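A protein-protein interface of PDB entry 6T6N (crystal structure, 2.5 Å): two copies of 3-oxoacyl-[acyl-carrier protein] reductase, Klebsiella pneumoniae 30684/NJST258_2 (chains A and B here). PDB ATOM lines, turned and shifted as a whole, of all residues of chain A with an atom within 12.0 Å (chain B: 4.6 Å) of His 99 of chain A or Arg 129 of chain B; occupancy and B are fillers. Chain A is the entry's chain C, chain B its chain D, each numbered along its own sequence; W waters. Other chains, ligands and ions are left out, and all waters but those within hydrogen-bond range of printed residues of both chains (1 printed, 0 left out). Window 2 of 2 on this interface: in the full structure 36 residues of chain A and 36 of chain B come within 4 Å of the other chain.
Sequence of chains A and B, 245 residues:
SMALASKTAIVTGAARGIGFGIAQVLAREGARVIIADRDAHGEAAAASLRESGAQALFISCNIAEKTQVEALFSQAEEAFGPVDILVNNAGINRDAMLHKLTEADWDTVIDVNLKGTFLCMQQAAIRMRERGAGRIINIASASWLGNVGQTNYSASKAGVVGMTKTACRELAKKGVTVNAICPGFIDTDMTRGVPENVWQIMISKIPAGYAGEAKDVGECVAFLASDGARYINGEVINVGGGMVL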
ATOM      1  N   ARG A  94       1.177  -7.287   2.043  1.00  0.00           N
ATOM      2  CA  ARG A  94       2.181  -6.471   1.353  1.00  0.00           C
ATOM      3  C   ARG A  94       3.177  -6.037   2.413  1.00  0.00           C
ATOM      4  O   ARG A  94       3.185  -4.898   2.870  1.00  0.00           O
ATOM      5  CB  ARG A  94       1.549  -5.264   0.686  1.00  0.00           C
ATOM      6  CG  ARG A  94       0.538  -5.593  -0.406  1.00  0.00           C
ATOM      7  CD  ARG A  94       1.186  -6.105  -1.674  1.00  0.00           C
ATOM      8  NE  ARG A  94       0.168  -6.283  -2.709  1.00  0.00           N
ATOM      9  CZ  ARG A  94      -0.517  -7.408  -2.944  1.00  0.00           C
ATOM     10  NH1 ARG A  94      -0.321  -8.523  -2.235  1.00  0.00           N
ATOM     11  NH2 ARG A  94      -1.429  -7.431  -3.900  1.00  0.00           N
ATOM     12  N   ASP A  95       4.001  -6.989   2.831  1.00  0.00           N
ATOM     13  CA  ASP A  95       4.871  -6.797   3.981  1.00  0.00           C
ATOM     14  C   ASP A  95       5.996  -5.809   3.686  1.00  0.00           C
ATOM     15  O   ASP A  95       6.413  -5.642   2.523  1.00  0.00           O
ATOM     16  CB  ASP A  95       5.457  -8.122   4.436  1.00  0.00           C
ATOM     17  CG  ASP A  95       4.392  -9.078   5.014  1.00  0.00           C
ATOM     18  OD1 ASP A  95       3.160  -8.745   5.060  1.00  0.00           O
ATOM     19  OD2 ASP A  95       4.811 -10.186   5.429  1.00  0.00           O
ATOM     20  N   ALA A  96       6.435  -5.138   4.752  1.00  0.00           N
ATOM     21  CA  ALA A  96       7.580  -4.248   4.742  1.00  0.00           C
ATOM     22  C   ALA A  96       7.798  -3.778   6.168  1.00  0.00           C
ATOM     23  O   ALA A  96       6.846  -3.641   6.941  1.00  0.00           O
ATOM     24  CB  ALA A  96       7.345  -3.043   3.852  1.00  0.00           C
ATOM     25  N   MET A  97       9.055  -3.483   6.484  1.00  0.00           N
ATOM     26  CA  MET A  97       9.416  -2.879   7.755  1.00  0.00           C
ATOM     27  C   MET A  97       8.744  -1.508   7.897  1.00  0.00           C
ATOM     28  O   MET A  97       8.436  -0.853   6.902  1.00  0.00           O
ATOM     29  CB  MET A  97      10.932  -2.752   7.856  1.00  0.00           C
ATOM     30  CG  MET A  97      11.676  -4.088   7.849  1.00  0.00           C
ATOM     31  SD  MET A  97      11.309  -5.128   9.280  1.00  0.00           S
ATOM     32  CE  MET A  97      12.221  -4.274  10.569  1.00  0.00           C
ATOM     33  N   LEU A  98       8.514  -1.088   9.136  1.00  0.00           N
ATOM     34  CA  LEU A  98       7.754   0.138   9.448  1.00  0.00           C
ATOM     35  C   LEU A  98       8.328   1.378   8.764  1.00  0.00           C
ATOM     36  O   LEU A  98       7.606   2.216   8.212  1.00  0.00           O
ATOM     37  CB  LEU A  98       7.696   0.354  10.963  1.00  0.00           C
ATOM     38  CG  LEU A  98       7.143   1.672  11.492  1.00  0.00           C
ATOM     39  CD1 LEU A  98       5.730   1.894  11.007  1.00  0.00           C
ATOM     40  CD2 LEU A  98       7.177   1.675  13.018  1.00  0.00           C
ATOM     41  N   HIS A  99       9.639   1.492   8.843  1.00  0.00           N
ATOM     42  CA  HIS A  99      10.387   2.584   8.220  1.00  0.00           C
ATOM     43  C   HIS A  99      10.432   2.582   6.686  1.00  0.00           C
ATOM     44  O   HIS A  99      10.779   3.593   6.111  1.00  0.00           O
ATOM     45  CB  HIS A  99      11.805   2.686   8.823  1.00  0.00           C
ATOM     46  CG  HIS A  99      12.702   1.535   8.492  1.00  0.00           C
ATOM     47  ND1 HIS A  99      12.564   0.282   9.060  1.00  0.00           N
ATOM     48  CD2 HIS A  99      13.779   1.458   7.672  1.00  0.00           C
ATOM     49  CE1 HIS A  99      13.510  -0.516   8.598  1.00  0.00           C
ATOM     50  NE2 HIS A  99      14.265   0.174   7.761  1.00  0.00           N
ATOM     51  N   LYS A 100      10.080   1.480   6.038  1.00  0.00           N
ATOM     52  CA  LYS A 100      10.096   1.359   4.563  1.00  0.00           C
ATOM     53  C   LYS A 100       8.728   1.263   3.877  1.00  0.00           C
ATOM     54  O   LYS A 100       8.643   1.422   2.667  1.00  0.00           O
ATOM     55  CB  LYS A 100      10.900   0.127   4.157  1.00  0.00           C
ATOM     56  CG  LYS A 100      12.379   0.183   4.508  1.00  0.00           C
ATOM     57  CD  LYS A 100      13.129  -0.882   3.698  1.00  0.00           C
ATOM     58  CE  LYS A 100      14.426  -1.383   4.344  1.00  0.00           C
ATOM     59  NZ  LYS A 100      15.491  -0.345   4.281  1.00  0.00           N
ATOM     60  N   LEU A 101       7.665   1.006   4.637  1.00  0.00           N
ATOM     61  CA  LEU A 101       6.375   0.674   4.051  1.00  0.00           C
ATOM     62  C   LEU A 101       5.840   1.816   3.201  1.00  0.00           C
ATOM     63  O   LEU A 101       5.711   2.942   3.685  1.00  0.00           O
ATOM     64  CB  LEU A 101       5.366   0.323   5.147  1.00  0.00           C
ATOM     65  CG  LEU A 101       3.942  -0.036   4.704  1.00  0.00           C
ATOM     66  CD1 LEU A 101       3.919  -1.332   3.920  1.00  0.00           C
ATOM     67  CD2 LEU A 101       3.014  -0.145   5.899  1.00  0.00           C
ATOM     68  N   THR A 102       5.517   1.521   1.940  1.00  0.00           N
ATOM     69  CA  THR A 102       5.002   2.548   1.047  1.00  0.00           C
ATOM     70  C   THR A 102       3.559   2.828   1.360  1.00  0.00           C
ATOM     71  O   THR A 102       2.846   1.970   1.885  1.00  0.00           O
ATOM     72  CB  THR A 102       5.103   2.167  -0.449  1.00  0.00           C
ATOM     73  OG1 THR A 102       4.260   1.040  -0.718  1.00  0.00           O
ATOM     74  CG2 THR A 102       6.567   1.880  -0.853  1.00  0.00           C
ATOM     75  N   GLU A 103       3.127   4.023   1.005  1.00  0.00           N
ATOM     76  CA  GLU A 103       1.745   4.417   1.182  1.00  0.00           C
ATOM     77  C   GLU A 103       0.786   3.507   0.403  1.00  0.00           C
ATOM     78  O   GLU A 103      -0.290   3.169   0.886  1.00  0.00           O
ATOM     79  CB  GLU A 103       1.574   5.883   0.781  1.00  0.00           C
ATOM     80  CG  GLU A 103       0.458   6.581   1.548  1.00  0.00           C
ATOM     81  CD  GLU A 103       0.327   8.060   1.236  1.00  0.00           C
ATOM     82  OE1 GLU A 103       1.259   8.670   0.654  1.00  0.00           O
ATOM     83  OE2 GLU A 103      -0.735   8.597   1.594  1.00  0.00           O
ATOM     84  N   ALA A 104       1.183   3.085  -0.787  1.00  0.00           N
ATOM     85  CA  ALA A 104       0.342   2.218  -1.631  1.00  0.00           C
ATOM     86  C   ALA A 104       0.152   0.855  -0.986  1.00  0.00           C
ATOM     87  O   ALA A 104      -0.959   0.306  -0.985  1.00  0.00           O
ATOM     88  CB  ALA A 104       0.952   2.057  -3.022  1.00  0.00           C
ATOM     89  N   ASP A 105       1.236   0.296  -0.447  1.00  0.00           N
ATOM     90  CA  ASP A 105       1.183  -1.011   0.203  1.00  0.00           C
ATOM     91  C   ASP A 105       0.395  -0.968   1.523  1.00  0.00           C
ATOM     92  O   ASP A 105      -0.271  -1.944   1.880  1.00  0.00           O
ATOM     93  CB  ASP A 105       2.596  -1.574   0.428  1.00  0.00           C
ATOM     94  CG  ASP A 105       3.222  -2.163  -0.845  1.00  0.00           C
ATOM     95  OD1 ASP A 105       2.510  -2.359  -1.867  1.00  0.00           O
ATOM     96  OD2 ASP A 105       4.452  -2.443  -0.812  1.00  0.00           O
ATOM     97  N   TRP A 106       0.479   0.150   2.248  1.00  0.00           N
ATOM     98  CA  TRP A 106      -0.389   0.380   3.393  1.00  0.00           C
ATOM     99  C   TRP A 106      -1.835   0.398   2.921  1.00  0.00           C
ATOM    100  O   TRP A 106      -2.655  -0.392   3.384  1.00  0.00           O
ATOM    101  CB  TRP A 106      -0.058   1.701   4.121  1.00  0.00           C
ATOM    102  CG  TRP A 106      -1.149   2.090   5.062  1.00  0.00           C
ATOM    103  CD1 TRP A 106      -2.252   2.831   4.766  1.00  0.00           C
ATOM    104  CD2 TRP A 106      -1.283   1.702   6.423  1.00  0.00           C
ATOM    105  NE1 TRP A 106      -3.062   2.939   5.855  1.00  0.00           N
ATOM    106  CE2 TRP A 106      -2.494   2.253   6.895  1.00  0.00           C
ATOM    107  CE3 TRP A 106      -0.498   0.946   7.299  1.00  0.00           C
ATOM    108  CZ2 TRP A 106      -2.944   2.064   8.196  1.00  0.00           C
ATOM    109  CZ3 TRP A 106      -0.943   0.755   8.598  1.00  0.00           C
ATOM    110  CH2 TRP A 106      -2.162   1.317   9.036  1.00  0.00           C
ATOM    111  N   ASN A 147       3.770  -8.571  14.546  1.00  0.00           N
ATOM    112  CA  ASN A 147       4.717  -9.395  13.831  1.00  0.00           C
ATOM    113  C   ASN A 147       5.645  -8.516  13.017  1.00  0.00           C
ATOM    114  O   ASN A 147       5.212  -7.561  12.370  1.00  0.00           O
ATOM    115  CB  ASN A 147       3.998 -10.349  12.900  1.00  0.00           C
ATOM    116  CG  ASN A 147       4.876 -11.499  12.442  1.00  0.00           C
ATOM    117  OD1 ASN A 147       5.834 -11.882  13.110  1.00  0.00           O
ATOM    118  ND2 ASN A 147       4.520 -12.083  11.317  1.00  0.00           N
ATOM    119  N   VAL A 148       6.920  -8.853  13.051  1.00  0.00           N
ATOM    120  CA  VAL A 148       7.943  -8.143  12.291  1.00  0.00           C
ATOM    121  C   VAL A 148       7.555  -8.066  10.809  1.00  0.00           C
ATOM    122  O   VAL A 148       7.130  -9.043  10.218  1.00  0.00           O
ATOM    123  CB  VAL A 148       9.319  -8.827  12.512  1.00  0.00           C
ATOM    124  CG1 VAL A 148      10.331  -8.404  11.476  1.00  0.00           C
ATOM    125  CG2 VAL A 148       9.833  -8.473  13.907  1.00  0.00           C
ATOM    126  N   GLY A 149       7.688  -6.886  10.228  1.00  0.00           N
ATOM    127  CA  GLY A 149       7.443  -6.693   8.798  1.00  0.00           C
ATOM    128  C   GLY A 149       5.976  -6.520   8.423  1.00  0.00           C
ATOM    129  O   GLY A 149       5.653  -6.481   7.227  1.00  0.00           O
ATOM    130  N   GLN A 150       5.092  -6.390   9.423  1.00  0.00           N
ATOM    131  CA  GLN A 150       3.667  -6.453   9.165  1.00  0.00           C
ATOM    132  C   GLN A 150       2.872  -5.336   9.842  1.00  0.00           C
ATOM    133  O   GLN A 150       1.790  -5.553  10.379  1.00  0.00           O
ATOM    134  CB  GLN A 150       3.157  -7.825   9.574  1.00  0.00           C
ATOM    135  CG  GLN A 150       3.745  -8.929   8.720  1.00  0.00           C
ATOM    136  CD  GLN A 150       3.017 -10.250   8.877  1.00  0.00           C
ATOM    137  OE1 GLN A 150       2.497 -10.584   9.948  1.00  0.00           O
ATOM    138  NE2 GLN A 150       2.976 -11.011   7.802  1.00  0.00           N
ATOM    139  N   THR A 151       3.400  -4.121   9.786  1.00  0.00           N
ATOM    140  CA  THR A 151       2.687  -2.971  10.305  1.00  0.00           C
ATOM    141  C   THR A 151       1.269  -2.885   9.686  1.00  0.00           C
ATOM    142  O   THR A 151       0.277  -2.764  10.404  1.00  0.00           O
ATOM    143  CB  THR A 151       3.475  -1.683  10.058  1.00  0.00           C
ATOM    144  OG1 THR A 151       4.643  -1.704  10.883  1.00  0.00           O
ATOM    145  CG2 THR A 151       2.638  -0.448  10.406  1.00  0.00           C
ATOM    146  N   ASN A 152       1.183  -2.967   8.365  1.00  0.00           N
ATOM    147  CA  ASN A 152      -0.107  -2.883   7.696  1.00  0.00           C
ATOM    148  C   ASN A 152      -1.003  -4.098   7.958  1.00  0.00           C
ATOM    149  O   ASN A 152      -2.195  -3.951   8.251  1.00  0.00           O
ATOM    150  CB  ASN A 152       0.040  -2.612   6.183  1.00  0.00           C
ATOM    151  CG  ASN A 152       0.935  -3.594   5.464  1.00  0.00           C
ATOM    152  OD1 ASN A 152       1.619  -4.423   6.057  1.00  0.00           O
ATOM    153  ND2 ASN A 152       0.946  -3.485   4.146  1.00  0.00           N
ATOM    154  N   SER A 154      -0.838  -6.433  10.474  1.00  0.00           N
ATOM    155  CA  SER A 154      -1.226  -6.523  11.875  1.00  0.00           C
ATOM    156  C   SER A 154      -2.299  -5.479  12.217  1.00  0.00           C
ATOM    157  O   SER A 154      -3.258  -5.779  12.916  1.00  0.00           O
ATOM    158  CB  SER A 154      -0.016  -6.390  12.808  1.00  0.00           C
ATOM    159  OG  SER A 154       0.547  -5.089  12.759  1.00  0.00           O
ATOM    160  N   GLN B 122       5.919   5.989  11.426  1.00  0.00           N
ATOM    161  CA  GLN B 122       6.902   5.763  10.376  1.00  0.00           C
ATOM    162  C   GLN B 122       8.008   6.815  10.388  1.00  0.00           C
ATOM    163  O   GLN B 122       9.199   6.475  10.347  1.00  0.00           O
ATOM    164  CB  GLN B 122       6.219   5.754   9.013  1.00  0.00           C
ATOM    165  CG  GLN B 122       7.175   5.595   7.855  1.00  0.00           C
ATOM    166  CD  GLN B 122       6.507   5.268   6.564  1.00  0.00           C
ATOM    167  OE1 GLN B 122       5.825   6.116   5.985  1.00  0.00           O
ATOM    168  NE2 GLN B 122       6.677   4.041   6.103  1.00  0.00           N
ATOM    169  N   ALA B 125      10.114   6.329  13.421  1.00  0.00           N
ATOM    170  CA  ALA B 125      10.893   5.102  13.303  1.00  0.00           C
ATOM    171  C   ALA B 125      12.123   5.283  12.415  1.00  0.00           C
ATOM    172  O   ALA B 125      13.206   4.830  12.775  1.00  0.00           O
ATOM    173  CB  ALA B 125      10.024   3.977  12.766  1.00  0.00           C
ATOM    174  N   ILE B 126      11.939   5.952  11.271  1.00  0.00           N
ATOM    175  CA  ILE B 126      13.031   6.262  10.346  1.00  0.00           C
ATOM    176  C   ILE B 126      14.192   6.940  11.078  1.00  0.00           C
ATOM    177  O   ILE B 126      15.361   6.586  10.862  1.00  0.00           O
ATOM    178  CB  ILE B 126      12.557   7.150   9.168  1.00  0.00           C
ATOM    179  CG1 ILE B 126      11.723   6.319   8.178  1.00  0.00           C
ATOM    180  CG2 ILE B 126      13.738   7.779   8.417  1.00  0.00           C
ATOM    181  CD1 ILE B 126      10.831   7.173   7.265  1.00  0.00           C
ATOM    182  N   ARG B 127      13.850   7.890  11.944  1.00  0.00           N
ATOM    183  CA  ARG B 127      14.826   8.667  12.687  1.00  0.00           C
ATOM    184  C   ARG B 127      15.359   7.924  13.902  1.00  0.00           C
ATOM    185  O   ARG B 127      16.570   7.820  14.084  1.00  0.00           O
ATOM    186  CB  ARG B 127      14.209   9.989  13.127  1.00  0.00           C
ATOM    187  CG  ARG B 127      13.941  10.915  11.956  1.00  0.00           C
ATOM    188  CD  ARG B 127      12.956  12.020  12.346  1.00  0.00           C
ATOM    189  NE  ARG B 127      12.801  13.012  11.281  1.00  0.00           N
ATOM    190  CZ  ARG B 127      12.096  12.856  10.175  1.00  0.00           C
ATOM    191  NH1 ARG B 127      11.401  11.744   9.933  1.00  0.00           N
ATOM    192  NH2 ARG B 127      12.081  13.838   9.284  1.00  0.00           N
ATOM    193  N   MET B 128      14.451   7.413  14.719  1.00  0.00           N
ATOM    194  CA  MET B 128      14.825   6.772  15.975  1.00  0.00           C
ATOM    195  C   MET B 128      15.686   5.525  15.810  1.00  0.00           C
ATOM    196  O   MET B 128      16.575   5.285  16.631  1.00  0.00           O
ATOM    197  CB  MET B 128      13.581   6.421  16.808  1.00  0.00           C
ATOM    198  CG  MET B 128      12.930   7.652  17.426  1.00  0.00           C
ATOM    199  SD  MET B 128      11.310   7.268  18.100  1.00  0.00           S
ATOM    200  CE  MET B 128      10.840   8.916  18.640  1.00  0.00           C
ATOM    201  N   ARG B 129      15.442   4.733  14.770  1.00  0.00           N
ATOM    202  CA  ARG B 129      16.249   3.530  14.567  1.00  0.00           C
ATOM    203  C   ARG B 129      17.724   3.827  14.231  1.00  0.00           C
ATOM    204  O   ARG B 129      18.598   3.045  14.601  1.00  0.00           O
ATOM    205  CB  ARG B 129      15.602   2.566  13.572  1.00  0.00           C
ATOM    206  CG  ARG B 129      15.751   2.920  12.101  1.00  0.00           C
ATOM    207  CD  ARG B 129      14.847   2.003  11.266  1.00  0.00           C
ATOM    208  NE  ARG B 129      15.245   0.586  11.358  1.00  0.00           N
ATOM    209  CZ  ARG B 129      16.263   0.030  10.689  1.00  0.00           C
ATOM    210  NH1 ARG B 129      17.012   0.743   9.849  1.00  0.00           N
ATOM    211  NH2 ARG B 129      16.525  -1.258  10.856  1.00  0.00           N
ATOM    212  N   GLU B 130      17.990   4.963  13.576  1.00  0.00           N
ATOM    213  CA  GLU B 130      19.371   5.438  13.337  1.00  0.00           C
ATOM    214  C   GLU B 130      20.031   6.012  14.591  1.00  0.00           C
ATOM    215  O   GLU B 130      21.213   5.804  14.798  1.00  0.00           O
ATOM    216  CB  GLU B 130      19.426   6.488  12.201  1.00  0.00           C
ATOM    217  CG  GLU B 130      18.887   6.035  10.841  1.00  0.00           C
ATOM    218  CD  GLU B 130      19.490   4.713  10.349  1.00  0.00           C
ATOM    219  OE1 GLU B 130      20.734   4.547  10.435  1.00  0.00           O
ATOM    220  OE2 GLU B 130      18.713   3.826   9.885  1.00  0.00           O
ATOM    221  N   ARG B 131      19.283   6.747  15.412  1.00  0.00           N
ATOM    222  CA  ARG B 131      19.819   7.338  16.661  1.00  0.00           C
ATOM    223  C   ARG B 131      20.052   6.333  17.779  1.00  0.00           C
ATOM    224  O   ARG B 131      20.792   6.629  18.708  1.00  0.00           O
ATOM    225  CB  ARG B 131      18.916   8.457  17.186  1.00  0.00           C
ATOM    226  CG  ARG B 131      19.184   9.797  16.514  1.00  0.00           C
ATOM    227  CD  ARG B 131      17.943  10.671  16.376  1.00  0.00           C
ATOM    228  NE  ARG B 131      17.934  11.401  15.102  1.00  0.00           N
ATOM    229  CZ  ARG B 131      16.926  12.161  14.660  1.00  0.00           C
ATOM    230  NH1 ARG B 131      15.813  12.301  15.383  1.00  0.00           N
ATOM    231  NH2 ARG B 131      17.025  12.783  13.487  1.00  0.00           N
ATOM    232  N   GLY B 132      19.408   5.165  17.719  1.00  0.00           N
ATOM    233  CA  GLY B 132      19.525   4.169  18.779  1.00  0.00           C
ATOM    234  C   GLY B 132      18.834   4.541  20.092  1.00  0.00           C
ATOM    235  O   GLY B 132      19.210   4.054  21.164  1.00  0.00           O
ATOM    236  N   LEU B 171      11.777  -2.460  16.651  1.00  0.00           N
ATOM    237  CA  LEU B 171      12.581  -1.354  17.144  1.00  0.00           C
ATOM    238  C   LEU B 171      13.191  -1.553  18.525  1.00  0.00           C
ATOM    239  O   LEU B 171      14.033  -0.745  18.931  1.00  0.00           O
ATOM    240  CB  LEU B 171      11.753  -0.064  17.157  1.00  0.00           C
ATOM    241  CG  LEU B 171      11.174   0.383  15.822  1.00  0.00           C
ATOM    242  CD1 LEU B 171      10.264   1.584  16.045  1.00  0.00           C
ATOM    243  CD2 LEU B 171      12.264   0.725  14.813  1.00  0.00           C
ATOM    244  N   LYS B 174      16.940  -1.628  18.843  1.00  0.00           N
ATOM    245  CA  LYS B 174      17.518  -0.309  18.593  1.00  0.00           C
ATOM    246  C   LYS B 174      17.363   0.685  19.770  1.00  0.00           C
ATOM    247  O   LYS B 174      17.573   1.883  19.578  1.00  0.00           O
ATOM    248  CB  LYS B 174      16.869   0.324  17.353  1.00  0.00           C
ATOM    249  CG  LYS B 174      16.794  -0.531  16.093  1.00  0.00           C
ATOM    250  CD  LYS B 174      18.162  -0.879  15.542  1.00  0.00           C
ATOM    251  CE  LYS B 174      18.002  -1.702  14.258  1.00  0.00           C
ATOM    252  NZ  LYS B 174      19.312  -1.828  13.554  1.00  0.00           N
HETATM  253  O   HOH W   1       4.419   5.613   3.791  1.00  0.00           O
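The side-chain amide nitrogen (NE2) of Gln 122 of chain B is in hydrogen-bond range of the backbone carbonyl oxygen (O) of Leu 101 of chain A, at 2.8 Å.
The backbone carbonyl oxygen (O) of Leu 98 of chain A lies within hydrogen-bond range of the side-chain amide nitrogen (NE2) of Gln 122 of chain B.
NE2 of His 99 of chain A is in hydrogen-bond range of NH1 of Arg 129 of chain B (3.5 Å).
NH1 of Arg 129 of chain B lies within salt-bridge range of OE2 of Glu 130 of chain B, 3.5 Å away.
Among the printed residues, pairs that only touch across the chains: Leu 98 of chain A with Ala 125 of chain B and His 99 of chain A with Ile 126 of chain B.
Of the printed residues of chain B, Leu 98 of chain A touches Gln 122 (2.9 Å) and Ala 125 (3.7 Å).
Of the printed residues of chain B, Leu 101 of chain A touches Gln 122.
Thr 102 of chain A touches none of the printed residues of chain B.
Thr 151 of chain A touches none of the printed residues of chain B.
Ala 125 of chain B touches one residue of chain A.
Ile 126 of chain B touches one residue of chain A.
Met 128 of chain B touches none of the printed residues of chain A.
No residue of chain A comes within 4 Å of Glu 130 of chain B.
No residue of chain A comes within 4 Å of Leu 171 of chain B.
The nearest residue of chain B that does not touch His 99 of chain A is Gln 122 of chain B (4.1 Å).
Of the 11 printed residues of chain B, 4 touch a printed residue of chain A.
Hydrophobic or aromatic side chains of chain B that line the printed part of chain A: Ala 125 and Ile 126.
Along chain B the printed residues that touch a printed residue of chain A span positions 122 to 129.
Hydrophobic or aromatic side chains of chain A within 4 Å of the printed part of chain B: Leu 98 and His 99.
Among the printed residues, 5 pairs touch across the chains.
Among the printed residues, no Asp or Glu carboxylate lies within 4 Å of a Lys or Arg side-chain nitrogen of the other chain.
No position is printed for both chains.
Water W1 lies within hydrogen-bond range of OE1 of Gln 122 of chain B (2.7 Å), O of Leu 101 of chain A (3.0 Å) and N of Glu 103 of chain A (3.5 Å).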
